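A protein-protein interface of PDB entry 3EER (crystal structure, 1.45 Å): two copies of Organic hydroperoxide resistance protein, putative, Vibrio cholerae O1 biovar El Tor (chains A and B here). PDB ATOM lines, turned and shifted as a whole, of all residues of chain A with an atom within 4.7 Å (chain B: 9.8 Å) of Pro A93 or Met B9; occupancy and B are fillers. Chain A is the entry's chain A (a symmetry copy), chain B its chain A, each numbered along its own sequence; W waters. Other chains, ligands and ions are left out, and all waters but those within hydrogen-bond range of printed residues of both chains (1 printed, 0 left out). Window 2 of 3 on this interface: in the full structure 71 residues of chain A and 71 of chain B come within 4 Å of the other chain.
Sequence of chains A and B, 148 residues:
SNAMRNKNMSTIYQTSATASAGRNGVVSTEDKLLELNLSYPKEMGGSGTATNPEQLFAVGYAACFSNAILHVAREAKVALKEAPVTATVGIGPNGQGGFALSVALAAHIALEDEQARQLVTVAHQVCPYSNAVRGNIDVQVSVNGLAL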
ATOM      1  N   GLY A  92     -21.576  24.693  25.942  1.00  0.00           N
ATOM      2  CA  GLY A  92     -20.841  23.998  26.957  1.00  0.00           C
ATOM      3  C   GLY A  92     -19.753  23.132  26.361  1.00  0.00           C
ATOM      4  O   GLY A  92     -19.666  22.966  25.139  1.00  0.00           O
ATOM      5  N   PRO A  93     -18.916  22.562  27.225  1.00  0.00           N
ATOM      6  CA  PRO A  93     -17.869  21.666  26.779  1.00  0.00           C
ATOM      7  C   PRO A  93     -18.424  20.419  26.144  1.00  0.00           C
ATOM      8  O   PRO A  93     -19.468  19.917  26.569  1.00  0.00           O
ATOM      9  CB  PRO A  93     -17.110  21.330  28.068  1.00  0.00           C
ATOM     10  CG  PRO A  93     -18.094  21.499  29.131  1.00  0.00           C
ATOM     11  CD  PRO A  93     -19.030  22.589  28.687  1.00  0.00           C
ATOM     12  N   ASN A  94     -17.747  19.897  25.127  1.00  0.00           N
ATOM     13  CA  ASN A  94     -18.204  18.660  24.488  1.00  0.00           C
ATOM     14  C   ASN A  94     -17.477  17.413  24.947  1.00  0.00           C
ATOM     15  O   ASN A  94     -17.774  16.329  24.451  1.00  0.00           O
ATOM     16  CB  ASN A  94     -18.180  18.786  22.955  1.00  0.00           C
ATOM     17  CG  ASN A  94     -16.778  18.933  22.379  1.00  0.00           C
ATOM     18  OD1 ASN A  94     -15.781  18.811  23.100  1.00  0.00           O
ATOM     19  ND2 ASN A  94     -16.697  19.192  21.081  1.00  0.00           N
ATOM     20  N   GLY A  95     -16.537  17.545  25.879  1.00  0.00           N
ATOM     21  CA  GLY A  95     -15.812  16.359  26.388  1.00  0.00           C
ATOM     22  C   GLY A  95     -14.756  15.852  25.426  1.00  0.00           C
ATOM     23  O   GLY A  95     -14.115  14.818  25.693  1.00  0.00           O
ATOM     24  N   GLY A  98     -13.390  20.613  23.008  1.00  0.00           N
ATOM     25  CA  GLY A  98     -14.016  21.771  22.396  1.00  0.00           C
ATOM     26  C   GLY A  98     -15.345  22.072  23.044  1.00  0.00           C
ATOM     27  O   GLY A  98     -15.584  21.770  24.248  1.00  0.00           O
ATOM     28  N   PHE A  99     -16.201  22.703  22.260  1.00  0.00           N
ATOM     29  CA  PHE A  99     -17.494  23.154  22.739  1.00  0.00           C
ATOM     30  C   PHE A  99     -18.552  22.816  21.726  1.00  0.00           C
ATOM     31  O   PHE A  99     -18.257  22.708  20.534  1.00  0.00           O
ATOM     32  CB  PHE A  99     -17.487  24.665  23.000  1.00  0.00           C
ATOM     33  CG  PHE A  99     -16.416  25.105  23.961  1.00  0.00           C
ATOM     34  CD1 PHE A  99     -16.690  25.177  25.325  1.00  0.00           C
ATOM     35  CD2 PHE A  99     -15.148  25.399  23.523  1.00  0.00           C
ATOM     36  CE1 PHE A  99     -15.700  25.574  26.228  1.00  0.00           C
ATOM     37  CE2 PHE A  99     -14.147  25.791  24.415  1.00  0.00           C
ATOM     38  CZ  PHE A  99     -14.427  25.866  25.766  1.00  0.00           C
ATOM     39  N   MET B   9     -21.437  18.335  28.014  1.00  0.00           N
ATOM     40  CA  MET B   9     -22.914  18.161  28.185  1.00  0.00           C
ATOM     41  C   MET B   9     -23.484  19.016  29.338  1.00  0.00           C
ATOM     42  O   MET B   9     -24.715  19.119  29.481  1.00  0.00           O
ATOM     43  CB  MET B   9     -23.268  16.703  28.404  1.00  0.00           C
ATOM     44  N   SER B  10     -22.605  19.633  30.138  1.00  0.00           N
ATOM     45  CA  SER B  10     -23.032  20.709  31.029  1.00  0.00           C
ATOM     46  C   SER B  10     -23.097  21.984  30.198  1.00  0.00           C
ATOM     47  O   SER B  10     -22.514  22.059  29.100  1.00  0.00           O
ATOM     48  CB  SER B  10     -22.065  20.882  32.189  1.00  0.00           C
ATOM     49  OG  SER B  10     -20.820  21.350  31.722  1.00  0.00           O
ATOM     50  N   THR B  11     -23.815  22.964  30.673  1.00  0.00           N
ATOM     51  CA  THR B  11     -23.995  24.217  29.971  1.00  0.00           C
ATOM     52  C   THR B  11     -23.369  25.324  30.804  1.00  0.00           C
ATOM     53  O   THR B  11     -23.663  25.453  31.972  1.00  0.00           O
ATOM     54  CB  THR B  11     -25.494  24.493  29.754  1.00  0.00           C
ATOM     55  OG1 THR B  11     -26.037  23.491  28.901  1.00  0.00           O
ATOM     56  CG2 THR B  11     -25.754  25.891  29.136  1.00  0.00           C
ATOM     57  N   ILE B  12     -22.471  26.072  30.200  1.00  0.00           N
ATOM     58  CA  ILE B  12     -21.834  27.162  30.939  1.00  0.00           C
ATOM     59  C   ILE B  12     -22.590  28.481  30.767  1.00  0.00           C
ATOM     60  O   ILE B  12     -22.547  29.310  31.656  1.00  0.00           O
ATOM     61  CB  ILE B  12     -20.338  27.286  30.624  1.00  0.00           C
ATOM     62  CG1 ILE B  12     -20.092  27.675  29.158  1.00  0.00           C
ATOM     63  CG2 ILE B  12     -19.651  25.967  30.934  1.00  0.00           C
ATOM     64  CD1 ILE B  12     -18.595  27.873  28.777  1.00  0.00           C
ATOM     65  N   TYR B  13     -23.303  28.660  29.666  1.00  0.00           N
ATOM     66  CA  TYR B  13     -24.037  29.910  29.391  1.00  0.00           C
ATOM     67  C   TYR B  13     -25.125  29.621  28.398  1.00  0.00           C
ATOM     68  O   TYR B  13     -24.930  28.907  27.436  1.00  0.00           O
ATOM     69  CB  TYR B  13     -23.082  30.985  28.839  1.00  0.00           C
ATOM     70  CG  TYR B  13     -23.753  32.218  28.311  1.00  0.00           C
ATOM     71  CD1 TYR B  13     -24.326  33.141  29.172  1.00  0.00           C
ATOM     72  CD2 TYR B  13     -23.820  32.472  26.944  1.00  0.00           C
ATOM     73  CE1 TYR B  13     -24.964  34.282  28.681  1.00  0.00           C
ATOM     74  CE2 TYR B  13     -24.426  33.590  26.455  1.00  0.00           C
ATOM     75  CZ  TYR B  13     -24.981  34.507  27.308  1.00  0.00           C
ATOM     76  OH  TYR B  13     -25.607  35.618  26.823  1.00  0.00           O
ATOM     77  N   GLN B  14     -26.285  30.234  28.616  1.00  0.00           N
ATOM     78  CA  GLN B  14     -27.349  30.181  27.622  1.00  0.00           C
ATOM     79  C   GLN B  14     -28.093  31.488  27.558  1.00  0.00           C
ATOM     80  O   GLN B  14     -28.087  32.273  28.513  1.00  0.00           O
ATOM     81  CB  GLN B  14     -28.309  29.037  27.847  1.00  0.00           C
ATOM     82  CG  GLN B  14     -28.946  29.009  29.149  1.00  0.00           C
ATOM     83  CD  GLN B  14     -29.814  27.747  29.341  1.00  0.00           C
ATOM     84  OE1 GLN B  14     -30.617  27.356  28.479  1.00  0.00           O
ATOM     85  NE2 GLN B  14     -29.625  27.101  30.460  1.00  0.00           N
ATOM     86  N   HIS B  71      -7.837  30.429  21.570  1.00  0.00           N
ATOM     87  CA  HIS B  71      -7.965  29.410  22.589  1.00  0.00           C
ATOM     88  C   HIS B  71      -6.962  28.282  22.355  1.00  0.00           C
ATOM     89  O   HIS B  71      -6.226  27.853  23.274  1.00  0.00           O
ATOM     90  CB  HIS B  71      -9.419  28.902  22.548  1.00  0.00           C
ATOM     91  CG  HIS B  71      -9.711  27.777  23.492  1.00  0.00           C
ATOM     92  ND1 HIS B  71     -10.362  27.951  24.694  1.00  0.00           N
ATOM     93  CD2 HIS B  71      -9.424  26.460  23.408  1.00  0.00           C
ATOM     94  CE1 HIS B  71     -10.467  26.780  25.306  1.00  0.00           C
ATOM     95  NE2 HIS B  71      -9.914  25.855  24.547  1.00  0.00           N
ATOM     96  N   VAL B 126     -12.472  22.365  17.486  1.00  0.00           N
ATOM     97  CA  VAL B 126     -12.854  22.848  18.803  1.00  0.00           C
ATOM     98  C   VAL B 126     -14.054  23.782  18.756  1.00  0.00           C
ATOM     99  O   VAL B 126     -14.877  23.798  19.675  1.00  0.00           O
ATOM    100  CB  VAL B 126     -11.622  23.641  19.446  1.00  0.00           C
ATOM    101  CG1 VAL B 126     -12.033  24.588  20.580  1.00  0.00           C
ATOM    102  CG2 VAL B 126     -10.560  22.633  19.891  1.00  0.00           C
ATOM    103  N   PRO B 128     -17.397  25.718  18.533  1.00  0.00           N
ATOM    104  CA  PRO B 128     -18.787  25.238  18.491  1.00  0.00           C
ATOM    105  C   PRO B 128     -19.524  25.590  17.202  1.00  0.00           C
ATOM    106  O   PRO B 128     -20.388  24.815  16.784  1.00  0.00           O
ATOM    107  CB  PRO B 128     -19.428  25.884  19.734  1.00  0.00           C
ATOM    108  CG  PRO B 128     -18.525  27.000  20.068  1.00  0.00           C
ATOM    109  CD  PRO B 128     -17.166  26.647  19.651  1.00  0.00           C
ATOM    110  N   ASN B 131     -18.356  22.894  14.826  1.00  0.00           N
ATOM    111  CA  ASN B 131     -18.990  21.653  15.224  1.00  0.00           C
ATOM    112  C   ASN B 131     -20.466  21.613  14.792  1.00  0.00           C
ATOM    113  O   ASN B 131     -20.984  20.561  14.435  1.00  0.00           O
ATOM    114  CB  ASN B 131     -18.840  21.399  16.722  1.00  0.00           C
ATOM    115  CG  ASN B 131     -17.427  21.008  17.137  1.00  0.00           C
ATOM    116  OD1 ASN B 131     -16.918  21.396  18.226  1.00  0.00           O
ATOM    117  ND2 ASN B 131     -16.830  20.188  16.359  1.00  0.00           N
HETATM  118  O   HOH W   1     -22.210  20.716  26.595  1.00  0.00           O
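Of the 6 printed residues of chain A, 5 touch a printed residue of chain B.
Printed residues of chain A that touch a printed residue of chain B: Gly A92, Pro A93, Asn A94, Gly A98 and Phe A99.
Hydrophobic or aromatic side chains of chain A that line the printed part of chain B: Pro A93 and Phe A99.
Among the printed residues, 9 pairs touch across the chains.
No position is printed for both chains.
Of the 9 pairs that touch across the chains among the printed residues, none has its exchanged pair printed and touching as well.
Among the printed residues, merely in contact across the chains: Gly A92 with Ser B10 (3.3 Å), Pro A93 with Ser B10 (3.5 Å), Asn A94 with Asn B131 (3.6 Å), Gly A98 with Val B126 (3.5 Å), Phe A99 with His B71 (3.9 Å) and Phe A99 with Pro B128 (3.3 Å).
Printed residues of chain B within 4 Å of Pro A93: Met B9 and Ser B10.
Of chain A, only Pro A93 (2.9 Å) comes within 4 Å of Met B9.
Asn A94 touches just one residue of chain B: Asn B131.
Printed residues of chain A within 4 Å of Ser B10: Gly A92 (3.3 Å) and Pro A93 (3.5 Å).
Printed residues of chain A within 4 Å of Asn B131: Asn A94 (3.6 Å) and Phe A99 (3.0 Å).
Ile B12 touches none of the printed residues of chain A.
The nearest printed residue of chain B that does not touch Pro A93 is Ile B12 (4.1 Å).
Water W1 lies within hydrogen-bond range of the backbone carbonyl oxygen of Pro A93 (2.9 Å), the backbone carbonyl oxygen of Ser B10 (2.9 Å) and the backbone NH of Met B9 (2.9 Å).
N of Met B9 is in hydrogen-bond range of O of Pro A93 (2.9 Å).
The backbone carbonyl oxygen of Val B126 is in hydrogen-bond range of the backbone NH of Phe A99, 3.1 Å away.
OD1 of Asn B131 lies close to O of Phe A99 (3.0 Å).
OD1 of Asn B131 lies close to O of Val B126, 3.5 Å away.
N of Gly A98 sits at hydrogen-bond distance from OD1 of Asn A94 (3.0 Å).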
